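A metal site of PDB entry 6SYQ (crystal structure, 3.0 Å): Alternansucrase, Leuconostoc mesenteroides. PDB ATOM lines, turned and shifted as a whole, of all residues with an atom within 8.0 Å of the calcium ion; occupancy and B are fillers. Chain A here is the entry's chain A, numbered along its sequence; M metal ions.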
ATOM      1  N   LYS A 419      27.431  -5.725  -4.659  1.00  0.00           N
ATOM      2  CA  LYS A 419      27.132  -6.166  -3.296  1.00  0.00           C
ATOM      3  C   LYS A 419      26.985  -7.671  -3.360  1.00  0.00           C
ATOM      4  O   LYS A 419      26.254  -8.182  -4.219  1.00  0.00           O
ATOM      5  CB  LYS A 419      25.862  -5.535  -2.809  1.00  0.00           C
ATOM      6  CG  LYS A 419      25.906  -4.026  -2.789  1.00  0.00           C
ATOM      7  CD  LYS A 419      24.519  -3.440  -2.827  1.00  0.00           C
ATOM      8  CE  LYS A 419      24.477  -2.139  -3.599  1.00  0.00           C
ATOM      9  NZ  LYS A 419      25.237  -1.118  -2.858  1.00  0.00           N
ATOM     10  N   LEU A 420      27.687  -8.372  -2.491  1.00  0.00           N
ATOM     11  CA  LEU A 420      27.695  -9.831  -2.557  1.00  0.00           C
ATOM     12  C   LEU A 420      26.869 -10.439  -1.451  1.00  0.00           C
ATOM     13  O   LEU A 420      26.819  -9.890  -0.336  1.00  0.00           O
ATOM     14  CB  LEU A 420      29.122 -10.333  -2.467  1.00  0.00           C
ATOM     15  CG  LEU A 420      30.067  -9.761  -3.523  1.00  0.00           C
ATOM     16  CD1 LEU A 420      31.410 -10.451  -3.352  1.00  0.00           C
ATOM     17  CD2 LEU A 420      29.556  -9.981  -4.923  1.00  0.00           C
ATOM     18  N   GLY A 421      26.179 -11.528  -1.774  1.00  0.00           N
ATOM     19  CA  GLY A 421      25.486 -12.319  -0.751  1.00  0.00           C
ATOM     20  C   GLY A 421      24.291 -11.649  -0.121  1.00  0.00           C
ATOM     21  O   GLY A 421      24.016 -11.842   1.072  1.00  0.00           O
ATOM     22  N   GLY A 438      25.185 -14.461   2.121  1.00  0.00           N
ATOM     23  CA  GLY A 438      24.825 -15.414   1.087  1.00  0.00           C
ATOM     24  C   GLY A 438      25.994 -15.899   0.273  1.00  0.00           C
ATOM     25  O   GLY A 438      26.938 -15.170   0.062  1.00  0.00           O
ATOM     26  N   SER A 439      25.942 -17.159  -0.144  1.00  0.00           N
ATOM     27  CA  SER A 439      26.945 -17.702  -1.035  1.00  0.00           C
ATOM     28  C   SER A 439      26.661 -17.201  -2.443  1.00  0.00           C
ATOM     29  O   SER A 439      25.999 -17.879  -3.195  1.00  0.00           O
ATOM     30  CB  SER A 439      26.894 -19.247  -1.001  1.00  0.00           C
ATOM     31  OG  SER A 439      26.844 -19.739   0.346  1.00  0.00           O
ATOM     32  N   GLU A 440      27.177 -16.027  -2.796  1.00  0.00           N
ATOM     33  CA  GLU A 440      26.843 -15.384  -4.075  1.00  0.00           C
ATOM     34  C   GLU A 440      27.373 -16.159  -5.247  1.00  0.00           C
ATOM     35  O   GLU A 440      26.812 -16.110  -6.353  1.00  0.00           O
ATOM     36  CB  GLU A 440      27.411 -13.968  -4.084  1.00  0.00           C
ATOM     37  CG  GLU A 440      27.101 -13.129  -5.327  1.00  0.00           C
ATOM     38  CD  GLU A 440      25.637 -12.799  -5.563  1.00  0.00           C
ATOM     39  OE1 GLU A 440      25.064 -11.993  -4.771  1.00  0.00           O
ATOM     40  OE2 GLU A 440      25.092 -13.319  -6.574  1.00  0.00           O
ATOM     41  N   PHE A 441      28.459 -16.895  -5.010  1.00  0.00           N
ATOM     42  CA  PHE A 441      29.167 -17.590  -6.093  1.00  0.00           C
ATOM     43  C   PHE A 441      28.792 -19.032  -6.117  1.00  0.00           C
ATOM     44  O   PHE A 441      28.855 -19.703  -5.082  1.00  0.00           O
ATOM     45  CB  PHE A 441      30.693 -17.474  -5.965  1.00  0.00           C
ATOM     46  CG  PHE A 441      31.185 -16.081  -6.079  1.00  0.00           C
ATOM     47  CD1 PHE A 441      31.435 -15.535  -7.313  1.00  0.00           C
ATOM     48  CD2 PHE A 441      31.339 -15.306  -4.963  1.00  0.00           C
ATOM     49  CE1 PHE A 441      31.859 -14.237  -7.428  1.00  0.00           C
ATOM     50  CE2 PHE A 441      31.775 -14.008  -5.060  1.00  0.00           C
ATOM     51  CZ  PHE A 441      32.027 -13.478  -6.300  1.00  0.00           C
ATOM     52  N   LEU A 442      28.402 -19.493  -7.305  1.00  0.00           N
ATOM     53  CA  LEU A 442      27.984 -20.841  -7.462  1.00  0.00           C
ATOM     54  C   LEU A 442      28.606 -21.477  -8.672  1.00  0.00           C
ATOM     55  O   LEU A 442      29.433 -22.388  -8.543  1.00  0.00           O
ATOM     56  CB  LEU A 442      26.451 -20.894  -7.533  1.00  0.00           C
ATOM     57  CG  LEU A 442      25.857 -22.295  -7.523  1.00  0.00           C
ATOM     58  CD1 LEU A 442      26.176 -23.046  -6.200  1.00  0.00           C
ATOM     59  CD2 LEU A 442      24.371 -22.157  -7.784  1.00  0.00           C
ATOM     60  N   LEU A 443      28.214 -21.018  -9.854  1.00  0.00           N
ATOM     61  CA  LEU A 443      28.729 -21.595 -11.101  1.00  0.00           C
ATOM     62  C   LEU A 443      29.069 -20.500 -12.085  1.00  0.00           C
ATOM     63  O   LEU A 443      28.419 -19.394 -12.115  1.00  0.00           O
ATOM     64  CB  LEU A 443      27.722 -22.549 -11.757  1.00  0.00           C
ATOM     65  CG  LEU A 443      27.629 -24.028 -11.436  1.00  0.00           C
ATOM     66  CD1 LEU A 443      28.980 -24.683 -11.562  1.00  0.00           C
ATOM     67  CD2 LEU A 443      27.077 -24.268 -10.057  1.00  0.00           C
ATOM     68  N   ASN A 445      30.077 -17.675 -14.617  1.00  0.00           N
ATOM     69  CA  ASN A 445      30.210 -16.239 -14.468  1.00  0.00           C
ATOM     70  C   ASN A 445      29.061 -15.737 -13.705  1.00  0.00           C
ATOM     71  O   ASN A 445      27.957 -15.843 -14.178  1.00  0.00           O
ATOM     72  CB  ASN A 445      30.185 -15.559 -15.821  1.00  0.00           C
ATOM     73  CG  ASN A 445      31.461 -15.765 -16.609  1.00  0.00           C
ATOM     74  OD1 ASN A 445      32.529 -15.240 -16.237  1.00  0.00           O
ATOM     75  ND2 ASN A 445      31.354 -16.501 -17.714  1.00  0.00           N
ATOM     76  N   ASP A 446      29.301 -15.214 -12.514  1.00  0.00           N
ATOM     77  CA  ASP A 446      28.225 -14.852 -11.631  1.00  0.00           C
ATOM     78  C   ASP A 446      27.821 -13.448 -11.966  1.00  0.00           C
ATOM     79  O   ASP A 446      28.626 -12.541 -11.901  1.00  0.00           O
ATOM     80  CB  ASP A 446      28.645 -15.029 -10.163  1.00  0.00           C
ATOM     81  CG  ASP A 446      27.537 -14.669  -9.178  1.00  0.00           C
ATOM     82  OD1 ASP A 446      26.674 -15.521  -8.886  1.00  0.00           O
ATOM     83  OD2 ASP A 446      27.556 -13.509  -8.694  1.00  0.00           O
ATOM     84  N   ILE A 447      26.563 -13.270 -12.349  1.00  0.00           N
ATOM     85  CA  ILE A 447      25.994 -11.983 -12.722  1.00  0.00           C
ATOM     86  C   ILE A 447      25.747 -11.128 -11.493  1.00  0.00           C
ATOM     87  O   ILE A 447      25.257 -11.613 -10.481  1.00  0.00           O
ATOM     88  CB  ILE A 447      24.678 -12.214 -13.476  1.00  0.00           C
ATOM     89  CG1 ILE A 447      24.986 -12.799 -14.858  1.00  0.00           C
ATOM     90  CG2 ILE A 447      23.847 -10.933 -13.635  1.00  0.00           C
ATOM     91  CD1 ILE A 447      23.818 -13.493 -15.522  1.00  0.00           C
ATOM     92  N   ASP A 448      26.061  -9.839 -11.605  1.00  0.00           N
ATOM     93  CA  ASP A 448      25.846  -8.858 -10.534  1.00  0.00           C
ATOM     94  C   ASP A 448      24.402  -8.355 -10.494  1.00  0.00           C
ATOM     95  O   ASP A 448      24.077  -7.295 -11.023  1.00  0.00           O
ATOM     96  CB  ASP A 448      26.812  -7.683 -10.695  1.00  0.00           C
ATOM     97  CG  ASP A 448      26.678  -6.647  -9.583  1.00  0.00           C
ATOM     98  OD1 ASP A 448      26.073  -6.957  -8.512  1.00  0.00           O
ATOM     99  OD2 ASP A 448      27.148  -5.499  -9.824  1.00  0.00           O
ATOM    100  N   ASN A 449      23.545  -9.125  -9.834  1.00  0.00           N
ATOM    101  CA  ASN A 449      22.137  -8.744  -9.683  1.00  0.00           C
ATOM    102  C   ASN A 449      21.903  -7.657  -8.617  1.00  0.00           C
ATOM    103  O   ASN A 449      20.751  -7.366  -8.323  1.00  0.00           O
ATOM    104  CB  ASN A 449      21.299  -9.989  -9.359  1.00  0.00           C
ATOM    105  CG  ASN A 449      21.320 -11.021 -10.470  1.00  0.00           C
ATOM    106  OD1 ASN A 449      21.089 -10.704 -11.624  1.00  0.00           O
ATOM    107  ND2 ASN A 449      21.621 -12.287 -10.121  1.00  0.00           N
ATOM    108  N   ALA A 487      18.082 -20.846  -7.765  1.00  0.00           N
ATOM    109  CA  ALA A 487      19.244 -20.407  -6.985  1.00  0.00           C
ATOM    110  C   ALA A 487      18.986 -19.080  -6.268  1.00  0.00           C
ATOM    111  O   ALA A 487      19.753 -18.131  -6.335  1.00  0.00           O
ATOM    112  CB  ALA A 487      20.481 -20.317  -7.881  1.00  0.00           C
ATOM    113  N   VAL A 488      17.894 -19.071  -5.526  1.00  0.00           N
ATOM    114  CA  VAL A 488      17.496 -17.907  -4.776  1.00  0.00           C
ATOM    115  C   VAL A 488      18.551 -17.387  -3.796  1.00  0.00           C
ATOM    116  O   VAL A 488      18.724 -16.160  -3.627  1.00  0.00           O
ATOM    117  CB  VAL A 488      16.203 -18.201  -4.013  1.00  0.00           C
ATOM    118  CG1 VAL A 488      15.843 -17.085  -3.025  1.00  0.00           C
ATOM    119  CG2 VAL A 488      15.070 -18.419  -5.020  1.00  0.00           C
ATOM    120  N   ASP A 489      19.224 -18.301  -3.105  1.00  0.00           N
ATOM    121  CA  ASP A 489      20.169 -17.913  -2.064  1.00  0.00           C
ATOM    122  C   ASP A 489      21.514 -17.466  -2.617  1.00  0.00           C
ATOM    123  O   ASP A 489      22.313 -16.869  -1.902  1.00  0.00           O
ATOM    124  CB  ASP A 489      20.303 -19.052  -1.060  1.00  0.00           C
ATOM    125  CG  ASP A 489      18.982 -19.315  -0.289  1.00  0.00           C
ATOM    126  OD1 ASP A 489      18.137 -18.393  -0.173  1.00  0.00           O
ATOM    127  OD2 ASP A 489      18.801 -20.445   0.227  1.00  0.00           O
ATOM    128  N   ASN A 490      21.705 -17.665  -3.904  1.00  0.00           N
ATOM    129  CA  ASN A 490      22.927 -17.240  -4.594  1.00  0.00           C
ATOM    130  C   ASN A 490      22.852 -15.934  -5.404  1.00  0.00           C
ATOM    131  O   ASN A 490      23.747 -15.660  -6.238  1.00  0.00           O
ATOM    132  CB  ASN A 490      23.348 -18.354  -5.521  1.00  0.00           C
ATOM    133  CG  ASN A 490      23.179 -19.706  -4.903  1.00  0.00           C
ATOM    134  OD1 ASN A 490      22.108 -20.279  -4.943  1.00  0.00           O
ATOM    135  ND2 ASN A 490      24.260 -20.217  -4.325  1.00  0.00           N
ATOM    136  N   VAL A 491      21.811 -15.155  -5.165  1.00  0.00           N
ATOM    137  CA  VAL A 491      21.547 -13.921  -5.872  1.00  0.00           C
ATOM    138  C   VAL A 491      20.988 -12.886  -4.915  1.00  0.00           C
ATOM    139  O   VAL A 491      20.733 -13.161  -3.746  1.00  0.00           O
ATOM    140  CB  VAL A 491      20.571 -14.076  -7.078  1.00  0.00           C
ATOM    141  CG1 VAL A 491      21.049 -15.148  -8.061  1.00  0.00           C
ATOM    142  CG2 VAL A 491      19.165 -14.363  -6.611  1.00  0.00           C
ATOM    143  N   ASP A 492      20.865 -11.680  -5.432  1.00  0.00           N
ATOM    144  CA  ASP A 492      20.343 -10.549  -4.669  1.00  0.00           C
ATOM    145  C   ASP A 492      18.845 -10.714  -4.546  1.00  0.00           C
ATOM    146  O   ASP A 492      18.128 -10.858  -5.533  1.00  0.00           O
ATOM    147  CB  ASP A 492      20.689  -9.226  -5.380  1.00  0.00           C
ATOM    148  CG  ASP A 492      20.442  -7.991  -4.512  1.00  0.00           C
ATOM    149  OD1 ASP A 492      19.359  -7.879  -3.896  1.00  0.00           O
ATOM    150  OD2 ASP A 492      21.302  -7.106  -4.484  1.00  0.00           O
ATOM    151  N   PRO A1023      18.650 -16.381 -13.255  1.00  0.00           N
ATOM    152  CA  PRO A1023      19.379 -15.123 -13.275  1.00  0.00           C
ATOM    153  C   PRO A1023      20.812 -15.139 -12.666  1.00  0.00           C
ATOM    154  O   PRO A1023      21.553 -14.147 -12.845  1.00  0.00           O
ATOM    155  CB  PRO A1023      18.461 -14.216 -12.451  1.00  0.00           C
ATOM    156  CG  PRO A1023      17.912 -15.136 -11.421  1.00  0.00           C
ATOM    157  CD  PRO A1023      17.730 -16.460 -12.121  1.00  0.00           C
ATOM    158  N   ASP A1024      21.205 -16.212 -11.978  1.00  0.00           N
ATOM    159  CA  ASP A1024      22.470 -16.204 -11.245  1.00  0.00           C
ATOM    160  C   ASP A1024      23.720 -16.194 -12.111  1.00  0.00           C
ATOM    161  O   ASP A1024      24.672 -15.488 -11.787  1.00  0.00           O
ATOM    162  CB  ASP A1024      22.569 -17.363 -10.281  1.00  0.00           C
ATOM    163  CG  ASP A1024      23.870 -17.358  -9.503  1.00  0.00           C
ATOM    164  OD1 ASP A1024      24.125 -16.385  -8.750  1.00  0.00           O
ATOM    165  OD2 ASP A1024      24.640 -18.303  -9.692  1.00  0.00           O
ATOM    166  N   GLN A1025      23.737 -16.937 -13.207  1.00  0.00           N
ATOM    167  CA  GLN A1025      24.946 -16.980 -14.018  1.00  0.00           C
ATOM    168  C   GLN A1025      24.749 -17.192 -15.527  1.00  0.00           C
ATOM    169  O   GLN A1025      23.635 -17.432 -16.013  1.00  0.00           O
ATOM    170  CB  GLN A1025      25.885 -18.064 -13.460  1.00  0.00           C
ATOM    171  CG  GLN A1025      25.522 -19.479 -13.854  1.00  0.00           C
ATOM    172  CD  GLN A1025      24.303 -19.998 -13.148  1.00  0.00           C
ATOM    173  OE1 GLN A1025      24.151 -19.768 -11.942  1.00  0.00           O
ATOM    174  NE2 GLN A1025      23.430 -20.699 -13.892  1.00  0.00           N
ATOM    175  N   GLU A1042      32.803 -19.159  -1.549  1.00  0.00           N
ATOM    176  CA  GLU A1042      31.437 -18.957  -2.087  1.00  0.00           C
ATOM    177  C   GLU A1042      30.750 -17.649  -1.668  1.00  0.00           C
ATOM    178  O   GLU A1042      29.957 -17.110  -2.430  1.00  0.00           O
ATOM    179  CB  GLU A1042      30.556 -20.139  -1.729  1.00  0.00           C
ATOM    180  CG  GLU A1042      30.249 -20.269  -0.241  1.00  0.00           C
ATOM    181  CD  GLU A1042      29.733 -21.640   0.137  1.00  0.00           C
ATOM    182  OE1 GLU A1042      30.438 -22.660  -0.028  1.00  0.00           O
ATOM    183  OE2 GLU A1042      28.582 -21.693   0.581  1.00  0.00           O
ATOM    184  N   ASN A1114      30.013 -10.315 -10.942  1.00  0.00           N
ATOM    185  CA  ASN A1114      30.662 -10.365  -9.653  1.00  0.00           C
ATOM    186  C   ASN A1114      31.942 -11.146  -9.707  1.00  0.00           C
ATOM    187  O   ASN A1114      32.873 -10.858  -8.964  1.00  0.00           O
ATOM    188  CB  ASN A1114      29.774 -11.015  -8.618  1.00  0.00           C
ATOM    189  CG  ASN A1114      28.576 -10.175  -8.268  1.00  0.00           C
ATOM    190  OD1 ASN A1114      28.646  -8.951  -8.311  1.00  0.00           O
ATOM    191  ND2 ASN A1114      27.454 -10.822  -7.896  1.00  0.00           N
ATOM    192  N   GLY A1115      31.989 -12.171 -10.550  1.00  0.00           N
ATOM    193  CA  GLY A1115      33.204 -12.959 -10.653  1.00  0.00           C
ATOM    194  C   GLY A1115      33.086 -14.141 -11.577  1.00  0.00           C
ATOM    195  O   GLY A1115      32.287 -14.151 -12.500  1.00  0.00           O
HETATM  196 CA    CA M   1      25.279 -14.875  -7.688  1.00  0.00          CA
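The side-chain carboxylate (OE1) of Glu 440 lies within hydrogen-bond range of the backbone NH (N) of Gly 421 (3.2 Å).
The backbone NH (N) of Glu 440 sits at hydrogen-bond distance from the backbone carbonyl oxygen (O) of Glu 1042 (3.0 Å).
The backbone carbonyl oxygen of Asp 446 sits at hydrogen-bond distance from the backbone NH of Asn 1114, at 2.8 Å.
The backbone carbonyl oxygen (O) of Gly 1115 lies within hydrogen-bond range of the backbone NH (N) of Asp 446.
The backbone carbonyl oxygen of Asp 1024 sits at hydrogen-bond distance from the backbone NH of Ile 447, at 3.0 Å.
OD2 of Asp 1024 lies close to OE1 of Gln 1025, at 2.7 Å.
The backbone carbonyl oxygen (O) of Ser 439 sits at hydrogen-bond distance from the side-chain amide nitrogen (ND2) of Asn 490 (3.1 Å).
The side-chain amide oxygen (OD1) of Asn 490 sits close to the backbone carbonyl oxygen (O) of Ala 487 (3.5 Å).
Four residues have an atom within 4 Å of the calcium ion: Glu 440, Asp 446, Asn 490 and Asp 1024.
The nearest printed residue that does not touch the calcium ion is Val 491 (4.3 Å).
OE2 of Glu 440 binds the calcium ion (1.9 Å).
The side-chain carboxylate (OD1) of Asp 446 is bound to the calcium ion, at 1.9 Å.
The calcium ion is bound by OD1 of Asp 1024.
O of Asn 490 is bound to the calcium ion.
O of Glu 440 binds the calcium ion (2.4 Å).
The calcium ion is bound by the side-chain carboxylate (OD2) of Asp 446 (2.8 Å).
The calcium ion has six donor atoms within binding distance.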
